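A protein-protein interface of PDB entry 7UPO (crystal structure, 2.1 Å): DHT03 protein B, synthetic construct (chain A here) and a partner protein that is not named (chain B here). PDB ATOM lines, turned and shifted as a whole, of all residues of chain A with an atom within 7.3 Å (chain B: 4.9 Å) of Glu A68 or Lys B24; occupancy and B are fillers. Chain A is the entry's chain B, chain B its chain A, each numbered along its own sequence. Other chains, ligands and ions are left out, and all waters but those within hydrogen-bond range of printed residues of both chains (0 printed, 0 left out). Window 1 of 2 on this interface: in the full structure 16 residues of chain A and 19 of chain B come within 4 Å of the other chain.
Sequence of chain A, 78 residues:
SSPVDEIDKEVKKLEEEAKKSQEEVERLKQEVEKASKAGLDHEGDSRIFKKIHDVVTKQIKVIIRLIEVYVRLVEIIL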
ATOM      1  N   ILE A   7       1.891  -4.853 -17.363  1.00  0.00           N
ATOM      2  CA  ILE A   7       0.511  -4.835 -16.893  1.00  0.00           C
ATOM      3  C   ILE A   7       0.056  -6.239 -16.522  1.00  0.00           C
ATOM      4  O   ILE A   7      -0.611  -6.439 -15.499  1.00  0.00           O
ATOM      5  CB  ILE A   7      -0.400  -4.196 -17.957  1.00  0.00           C
ATOM      6  CG1 ILE A   7      -0.144  -2.691 -18.013  1.00  0.00           C
ATOM      7  CG2 ILE A   7      -1.863  -4.498 -17.671  1.00  0.00           C
ATOM      8  CD1 ILE A   7      -1.181  -1.929 -18.770  1.00  0.00           C
ATOM      9  N   LEU A  14      -2.335  -7.906  -8.326  1.00  0.00           N
ATOM     10  CA  LEU A  14      -3.645  -7.508  -7.821  1.00  0.00           C
ATOM     11  C   LEU A  14      -4.572  -8.705  -7.659  1.00  0.00           C
ATOM     12  O   LEU A  14      -5.429  -8.706  -6.769  1.00  0.00           O
ATOM     13  CB  LEU A  14      -4.277  -6.472  -8.749  1.00  0.00           C
ATOM     14  CG  LEU A  14      -3.588  -5.107  -8.782  1.00  0.00           C
ATOM     15  CD1 LEU A  14      -4.273  -4.187  -9.774  1.00  0.00           C
ATOM     16  CD2 LEU A  14      -3.579  -4.490  -7.394  1.00  0.00           C
ATOM     17  N   LYS A  61     -10.793  -0.454  -2.709  1.00  0.00           N
ATOM     18  CA  LYS A  61      -9.488   0.059  -3.111  1.00  0.00           C
ATOM     19  C   LYS A  61      -8.747  -0.935  -3.996  1.00  0.00           C
ATOM     20  O   LYS A  61      -7.987  -0.529  -4.883  1.00  0.00           O
ATOM     21  CB  LYS A  61      -8.657   0.406  -1.876  1.00  0.00           C
ATOM     22  CG  LYS A  61      -9.099   1.678  -1.168  1.00  0.00           C
ATOM     23  CD  LYS A  61      -8.235   1.959   0.050  1.00  0.00           C
ATOM     24  CE  LYS A  61      -8.614   3.277   0.703  1.00  0.00           C
ATOM     25  NZ  LYS A  61      -7.809   3.539   1.927  1.00  0.00           N
ATOM     26  N   VAL A  62      -8.952  -2.234  -3.773  1.00  0.00           N
ATOM     27  CA  VAL A  62      -8.393  -3.231  -4.680  1.00  0.00           C
ATOM     28  C   VAL A  62      -9.047  -3.122  -6.051  1.00  0.00           C
ATOM     29  O   VAL A  62      -8.385  -3.277  -7.084  1.00  0.00           O
ATOM     30  CB  VAL A  62      -8.544  -4.642  -4.085  1.00  0.00           C
ATOM     31  CG1 VAL A  62      -8.041  -5.695  -5.063  1.00  0.00           C
ATOM     32  CG2 VAL A  62      -7.791  -4.742  -2.767  1.00  0.00           C
ATOM     33  N   ILE A  63     -10.352  -2.840  -6.082  1.00  0.00           N
ATOM     34  CA  ILE A  63     -11.053  -2.670  -7.351  1.00  0.00           C
ATOM     35  C   ILE A  63     -10.519  -1.448  -8.091  1.00  0.00           C
ATOM     36  O   ILE A  63     -10.291  -1.486  -9.306  1.00  0.00           O
ATOM     37  CB  ILE A  63     -12.571  -2.561  -7.120  1.00  0.00           C
ATOM     38  CG1 ILE A  63     -13.117  -3.843  -6.490  1.00  0.00           C
ATOM     39  CG2 ILE A  63     -13.282  -2.254  -8.426  1.00  0.00           C
ATOM     40  CD1 ILE A  63     -14.590  -3.771  -6.154  1.00  0.00           C
ATOM     41  N   ILE A  64     -10.318  -0.346  -7.364  1.00  0.00           N
ATOM     42  CA  ILE A  64      -9.845   0.889  -7.987  1.00  0.00           C
ATOM     43  C   ILE A  64      -8.467   0.684  -8.605  1.00  0.00           C
ATOM     44  O   ILE A  64      -8.203   1.130  -9.729  1.00  0.00           O
ATOM     45  CB  ILE A  64      -9.846   2.033  -6.957  1.00  0.00           C
ATOM     46  CG1 ILE A  64     -11.283   2.402  -6.577  1.00  0.00           C
ATOM     47  CG2 ILE A  64      -9.094   3.244  -7.495  1.00  0.00           C
ATOM     48  CD1 ILE A  64     -11.384   3.458  -5.494  1.00  0.00           C
ATOM     49  N   ARG A  65      -7.569   0.004  -7.888  1.00  0.00           N
ATOM     50  CA  ARG A  65      -6.249  -0.272  -8.445  1.00  0.00           C
ATOM     51  C   ARG A  65      -6.350  -1.150  -9.686  1.00  0.00           C
ATOM     52  O   ARG A  65      -5.591  -0.969 -10.645  1.00  0.00           O
ATOM     53  CB  ARG A  65      -5.354  -0.919  -7.391  1.00  0.00           C
ATOM     54  CG  ARG A  65      -4.990   0.010  -6.243  1.00  0.00           C
ATOM     55  CD  ARG A  65      -3.800  -0.513  -5.450  1.00  0.00           C
ATOM     56  NE  ARG A  65      -4.073  -1.804  -4.828  1.00  0.00           N
ATOM     57  CZ  ARG A  65      -4.713  -1.955  -3.673  1.00  0.00           C
ATOM     58  NH1 ARG A  65      -5.153  -0.893  -3.011  1.00  0.00           N
ATOM     59  NH2 ARG A  65      -4.915  -3.169  -3.179  1.00  0.00           N
ATOM     60  N   LEU A  66      -7.292  -2.099  -9.691  1.00  0.00           N
ATOM     61  CA  LEU A  66      -7.533  -2.894 -10.891  1.00  0.00           C
ATOM     62  C   LEU A  66      -7.965  -2.016 -12.058  1.00  0.00           C
ATOM     63  O   LEU A  66      -7.492  -2.194 -13.187  1.00  0.00           O
ATOM     64  CB  LEU A  66      -8.592  -3.960 -10.614  1.00  0.00           C
ATOM     65  CG  LEU A  66      -8.114  -5.347 -10.193  1.00  0.00           C
ATOM     66  CD1 LEU A  66      -9.310  -6.237  -9.912  1.00  0.00           C
ATOM     67  CD2 LEU A  66      -7.231  -5.958 -11.273  1.00  0.00           C
ATOM     68  N   ILE A  67      -8.866  -1.065 -11.804  1.00  0.00           N
ATOM     69  CA  ILE A  67      -9.357  -0.202 -12.873  1.00  0.00           C
ATOM     70  C   ILE A  67      -8.246   0.707 -13.381  1.00  0.00           C
ATOM     71  O   ILE A  67      -8.107   0.921 -14.591  1.00  0.00           O
ATOM     72  CB  ILE A  67     -10.576   0.604 -12.387  1.00  0.00           C
ATOM     73  CG1 ILE A  67     -11.714  -0.341 -11.997  1.00  0.00           C
ATOM     74  CG2 ILE A  67     -11.031   1.582 -13.455  1.00  0.00           C
ATOM     75  CD1 ILE A  67     -12.920   0.358 -11.415  1.00  0.00           C
ATOM     76  N   GLU A  68      -7.436   1.253 -12.470  1.00  0.00           N
ATOM     77  CA  GLU A  68      -6.324   2.097 -12.894  1.00  0.00           C
ATOM     78  C   GLU A  68      -5.315   1.313 -13.721  1.00  0.00           C
ATOM     79  O   GLU A  68      -4.698   1.869 -14.637  1.00  0.00           O
ATOM     80  CB  GLU A  68      -5.653   2.730 -11.676  1.00  0.00           C
ATOM     81  CG  GLU A  68      -6.547   3.702 -10.923  1.00  0.00           C
ATOM     82  CD  GLU A  68      -5.934   4.176  -9.622  1.00  0.00           C
ATOM     83  OE1 GLU A  68      -4.965   3.540  -9.155  1.00  0.00           O
ATOM     84  OE2 GLU A  68      -6.416   5.185  -9.063  1.00  0.00           O
ATOM     85  N   VAL A  69      -5.131   0.028 -13.412  1.00  0.00           N
ATOM     86  CA  VAL A  69      -4.343  -0.835 -14.284  1.00  0.00           C
ATOM     87  C   VAL A  69      -5.077  -1.058 -15.600  1.00  0.00           C
ATOM     88  O   VAL A  69      -4.481  -0.986 -16.683  1.00  0.00           O
ATOM     89  CB  VAL A  69      -4.029  -2.160 -13.569  1.00  0.00           C
ATOM     90  CG1 VAL A  69      -3.524  -3.196 -14.556  1.00  0.00           C
ATOM     91  CG2 VAL A  69      -3.008  -1.931 -12.465  1.00  0.00           C
ATOM     92  N   TYR A  70      -6.385  -1.315 -15.522  1.00  0.00           N
ATOM     93  CA  TYR A  70      -7.205  -1.456 -16.720  1.00  0.00           C
ATOM     94  C   TYR A  70      -7.078  -0.234 -17.622  1.00  0.00           C
ATOM     95  O   TYR A  70      -6.942  -0.367 -18.844  1.00  0.00           O
ATOM     96  CB  TYR A  70      -8.661  -1.679 -16.311  1.00  0.00           C
ATOM     97  CG  TYR A  70      -9.580  -2.162 -17.407  1.00  0.00           C
ATOM     98  CD1 TYR A  70      -9.079  -2.716 -18.578  1.00  0.00           C
ATOM     99  CD2 TYR A  70     -10.958  -2.061 -17.266  1.00  0.00           C
ATOM    100  CE1 TYR A  70      -9.928  -3.157 -19.576  1.00  0.00           C
ATOM    101  CE2 TYR A  70     -11.811  -2.496 -18.256  1.00  0.00           C
ATOM    102  CZ  TYR A  70     -11.294  -3.043 -19.407  1.00  0.00           C
ATOM    103  OH  TYR A  70     -12.151  -3.476 -20.392  1.00  0.00           O
ATOM    104  N   VAL A  71      -7.106   0.966 -17.032  1.00  0.00           N
ATOM    105  CA  VAL A  71      -6.975   2.194 -17.815  1.00  0.00           C
ATOM    106  C   VAL A  71      -5.631   2.233 -18.527  1.00  0.00           C
ATOM    107  O   VAL A  71      -5.545   2.612 -19.701  1.00  0.00           O
ATOM    108  CB  VAL A  71      -7.173   3.426 -16.911  1.00  0.00           C
ATOM    109  CG1 VAL A  71      -6.806   4.705 -17.655  1.00  0.00           C
ATOM    110  CG2 VAL A  71      -8.607   3.496 -16.423  1.00  0.00           C
ATOM    111  N   ARG A  72      -4.561   1.842 -17.829  1.00  0.00           N
ATOM    112  CA  ARG A  72      -3.243   1.802 -18.454  1.00  0.00           C
ATOM    113  C   ARG A  72      -3.227   0.846 -19.639  1.00  0.00           C
ATOM    114  O   ARG A  72      -2.556   1.105 -20.646  1.00  0.00           O
ATOM    115  CB  ARG A  72      -2.188   1.401 -17.425  1.00  0.00           C
ATOM    116  CG  ARG A  72      -1.888   2.472 -16.391  1.00  0.00           C
ATOM    117  CD  ARG A  72      -1.259   1.865 -15.149  1.00  0.00           C
ATOM    118  NE  ARG A  72      -0.159   0.962 -15.476  1.00  0.00           N
ATOM    119  CZ  ARG A  72       0.441   0.168 -14.594  1.00  0.00           C
ATOM    120  NH1 ARG A  72       0.047   0.163 -13.329  1.00  0.00           N
ATOM    121  NH2 ARG A  72       1.436  -0.623 -14.979  1.00  0.00           N
ATOM    122  N   LEU A  73      -3.966  -0.261 -19.542  1.00  0.00           N
ATOM    123  CA  LEU A  73      -4.051  -1.198 -20.658  1.00  0.00           C
ATOM    124  C   LEU A  73      -4.694  -0.547 -21.873  1.00  0.00           C
ATOM    125  O   LEU A  73      -4.271  -0.781 -23.011  1.00  0.00           O
ATOM    126  CB  LEU A  73      -4.836  -2.440 -20.239  1.00  0.00           C
ATOM    127  CG  LEU A  73      -5.000  -3.524 -21.303  1.00  0.00           C
ATOM    128  CD1 LEU A  73      -3.644  -4.090 -21.690  1.00  0.00           C
ATOM    129  CD2 LEU A  73      -5.925  -4.625 -20.810  1.00  0.00           C
ATOM    130  N   VAL A  74      -5.714   0.281 -21.650  1.00  0.00           N
ATOM    131  CA  VAL A  74      -6.393   0.944 -22.758  1.00  0.00           C
ATOM    132  C   VAL A  74      -5.486   1.992 -23.390  1.00  0.00           C
ATOM    133  O   VAL A  74      -5.442   2.137 -24.617  1.00  0.00           O
ATOM    134  CB  VAL A  74      -7.718   1.560 -22.274  1.00  0.00           C
ATOM    135  CG1 VAL A  74      -8.525   2.053 -23.451  1.00  0.00           C
ATOM    136  CG2 VAL A  74      -8.511   0.549 -21.459  1.00  0.00           C
ATOM    137  N   GLU A  75      -4.747   2.737 -22.565  1.00  0.00           N
ATOM    138  CA  GLU A  75      -3.883   3.794 -23.078  1.00  0.00           C
ATOM    139  C   GLU A  75      -2.681   3.249 -23.834  1.00  0.00           C
ATOM    140  O   GLU A  75      -2.100   3.973 -24.649  1.00  0.00           O
ATOM    141  CB  GLU A  75      -3.415   4.688 -21.931  1.00  0.00           C
ATOM    142  CG  GLU A  75      -4.544   5.392 -21.201  1.00  0.00           C
ATOM    143  CD  GLU A  75      -4.073   6.113 -19.955  1.00  0.00           C
ATOM    144  OE1 GLU A  75      -2.990   5.765 -19.440  1.00  0.00           O
ATOM    145  OE2 GLU A  75      -4.786   7.030 -19.493  1.00  0.00           O
ATOM    146  N   LEU B  20     -13.367   7.912 -10.688  1.00  0.00           N
ATOM    147  CA  LEU B  20     -12.449   7.315  -9.725  1.00  0.00           C
ATOM    148  C   LEU B  20     -11.993   8.339  -8.694  1.00  0.00           C
ATOM    149  O   LEU B  20     -11.937   8.047  -7.493  1.00  0.00           O
ATOM    150  CB  LEU B  20     -11.248   6.710 -10.451  1.00  0.00           C
ATOM    151  CG  LEU B  20     -11.508   5.438 -11.256  1.00  0.00           C
ATOM    152  CD1 LEU B  20     -10.268   5.037 -12.035  1.00  0.00           C
ATOM    153  CD2 LEU B  20     -11.943   4.313 -10.332  1.00  0.00           C
ATOM    154  N   ASP B  21     -11.663   9.550  -9.149  1.00  0.00           N
ATOM    155  CA  ASP B  21     -11.223  10.597  -8.233  1.00  0.00           C
ATOM    156  C   ASP B  21     -12.294  10.902  -7.192  1.00  0.00           C
ATOM    157  O   ASP B  21     -12.016  10.920  -5.986  1.00  0.00           O
ATOM    158  CB  ASP B  21     -10.861  11.858  -9.021  1.00  0.00           C
ATOM    159  CG  ASP B  21     -10.297  12.959  -8.140  1.00  0.00           C
ATOM    160  OD1 ASP B  21      -9.949  12.679  -6.973  1.00  0.00           O
ATOM    161  OD2 ASP B  21     -10.205  14.110  -8.616  1.00  0.00           O
ATOM    162  N   ARG B  22     -13.530  11.133  -7.639  1.00  0.00           N
ATOM    163  CA  ARG B  22     -14.594  11.448  -6.693  1.00  0.00           C
ATOM    164  C   ARG B  22     -14.957  10.243  -5.836  1.00  0.00           C
ATOM    165  O   ARG B  22     -15.417  10.408  -4.699  1.00  0.00           O
ATOM    166  CB  ARG B  22     -15.831  11.966  -7.428  1.00  0.00           C
ATOM    167  CG  ARG B  22     -16.820  12.653  -6.505  1.00  0.00           C
ATOM    168  CD  ARG B  22     -18.227  12.649  -7.065  1.00  0.00           C
ATOM    169  NE  ARG B  22     -19.206  12.961  -6.028  1.00  0.00           N
ATOM    170  CZ  ARG B  22     -20.522  12.876  -6.189  1.00  0.00           C
ATOM    171  NH1 ARG B  22     -21.026  12.486  -7.352  1.00  0.00           N
ATOM    172  NH2 ARG B  22     -21.334  13.178  -5.185  1.00  0.00           N
ATOM    173  N   LEU B  23     -14.762   9.028  -6.355  1.00  0.00           N
ATOM    174  CA  LEU B  23     -15.011   7.839  -5.548  1.00  0.00           C
ATOM    175  C   LEU B  23     -14.026   7.749  -4.388  1.00  0.00           C
ATOM    176  O   LEU B  23     -14.415   7.424  -3.260  1.00  0.00           O
ATOM    177  CB  LEU B  23     -14.936   6.585  -6.418  1.00  0.00           C
ATOM    178  CG  LEU B  23     -15.152   5.252  -5.702  1.00  0.00           C
ATOM    179  CD1 LEU B  23     -16.478   5.248  -4.963  1.00  0.00           C
ATOM    180  CD2 LEU B  23     -15.084   4.099  -6.689  1.00  0.00           C
ATOM    181  N   LYS B  24     -12.748   8.040  -4.645  1.00  0.00           N
ATOM    182  CA  LYS B  24     -11.756   8.018  -3.574  1.00  0.00           C
ATOM    183  C   LYS B  24     -12.036   9.101  -2.541  1.00  0.00           C
ATOM    184  O   LYS B  24     -11.796   8.901  -1.345  1.00  0.00           O
ATOM    185  CB  LYS B  24     -10.350   8.170  -4.154  1.00  0.00           C
ATOM    186  CG  LYS B  24      -9.786   6.878  -4.727  1.00  0.00           C
ATOM    187  CD  LYS B  24      -8.382   7.065  -5.289  1.00  0.00           C
ATOM    188  CE  LYS B  24      -8.404   7.813  -6.610  1.00  0.00           C
ATOM    189  NZ  LYS B  24      -7.052   7.870  -7.237  1.00  0.00           N
ATOM    190  N   LYS B  25     -12.543  10.257  -2.982  1.00  0.00           N
ATOM    191  CA  LYS B  25     -12.928  11.296  -2.033  1.00  0.00           C
ATOM    192  C   LYS B  25     -14.072  10.829  -1.142  1.00  0.00           C
ATOM    193  O   LYS B  25     -14.121  11.166   0.047  1.00  0.00           O
ATOM    194  CB  LYS B  25     -13.317  12.575  -2.776  1.00  0.00           C
ATOM    195  CG  LYS B  25     -12.162  13.276  -3.471  1.00  0.00           C
ATOM    196  CD  LYS B  25     -12.630  14.539  -4.174  1.00  0.00           C
ATOM    197  CE  LYS B  25     -11.484  15.235  -4.893  1.00  0.00           C
ATOM    198  NZ  LYS B  25     -11.952  16.440  -5.632  1.00  0.00           N
ATOM    199  N   ILE B  26     -15.002  10.049  -1.701  1.00  0.00           N
ATOM    200  CA  ILE B  26     -16.121   9.545  -0.911  1.00  0.00           C
ATOM    201  C   ILE B  26     -15.636   8.537   0.121  1.00  0.00           C
ATOM    202  O   ILE B  26     -16.052   8.575   1.285  1.00  0.00           O
ATOM    203  CB  ILE B  26     -17.194   8.938  -1.833  1.00  0.00           C
ATOM    204  CG1 ILE B  26     -17.871  10.034  -2.650  1.00  0.00           C
ATOM    205  CG2 ILE B  26     -18.224   8.163  -1.023  1.00  0.00           C
ATOM    206  CD1 ILE B  26     -18.984   9.524  -3.513  1.00  0.00           C
ATOM    207  N   LEU B  27     -14.756   7.620  -0.287  1.00  0.00           N
ATOM    208  CA  LEU B  27     -14.216   6.648   0.658  1.00  0.00           C
ATOM    209  C   LEU B  27     -13.477   7.339   1.794  1.00  0.00           C
ATOM    210  O   LEU B  27     -13.542   6.897   2.947  1.00  0.00           O
ATOM    211  CB  LEU B  27     -13.289   5.669  -0.065  1.00  0.00           C
ATOM    212  CG  LEU B  27     -13.931   4.716  -1.074  1.00  0.00           C
ATOM    213  CD1 LEU B  27     -12.864   3.875  -1.754  1.00  0.00           C
ATOM    214  CD2 LEU B  27     -14.961   3.827  -0.397  1.00  0.00           C
ATOM    215  N   GLU B  28     -12.775   8.433   1.491  1.00  0.00           N
ATOM    216  CA  GLU B  28     -12.058   9.162   2.531  1.00  0.00           C
ATOM    217  C   GLU B  28     -13.020   9.896   3.457  1.00  0.00           C
ATOM    218  O   GLU B  28     -12.826   9.904   4.678  1.00  0.00           O
ATOM    219  CB  GLU B  28     -11.071  10.143   1.903  1.00  0.00           C
ATOM    220  CG  GLU B  28     -10.227  10.889   2.920  1.00  0.00           C
ATOM    221  CD  GLU B  28      -9.502  12.072   2.316  1.00  0.00           C
ATOM    222  OE1 GLU B  28      -9.719  12.353   1.118  1.00  0.00           O
ATOM    223  OE2 GLU B  28      -8.717  12.724   3.037  1.00  0.00           O
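The side-chain amino group of Lys B24 lies within salt-bridge range of the side-chain carboxylate of Glu A68 (3.3 Å).
Ile A64 touches Leu B23. CD1 of Ile A64 touches CG of Lys B24 (3.9 Å). Ile A67 touches Leu B20.
Of chain B, only Lys B24 comes within 4 Å of Glu A68. Printed residues of chain A within 4 Å of Lys B24: Ile A64 and Glu A68. Of the printed residues of chain B, Ile A64 touches Leu B23 (3.9 Å) and Lys B24 (3.9 Å). Printed residues of chain A within 4 Å of Leu B20: Ile A67 (3.8 Å). Ile A7 touches none of the printed residues of chain B. The nearest residue of chain B that does not touch Glu A68 is Leu B20 (4.1 Å). The nearest printed residue of chain B that does not touch Ile A64 is Leu B27 (4.04 Å).
Of the 9 printed residues of chain B, 3 touch a printed residue of chain A. Printed residues of chain B that touch a printed residue of chain A: Leu B20, Leu B23 and Lys B24. Of the 17 printed residues of chain A, 3 touch a printed residue of chain B. Hydrophobic or aromatic side chains of chain A within 4 Å of the printed part of chain B: Ile A64 and Ile A67.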
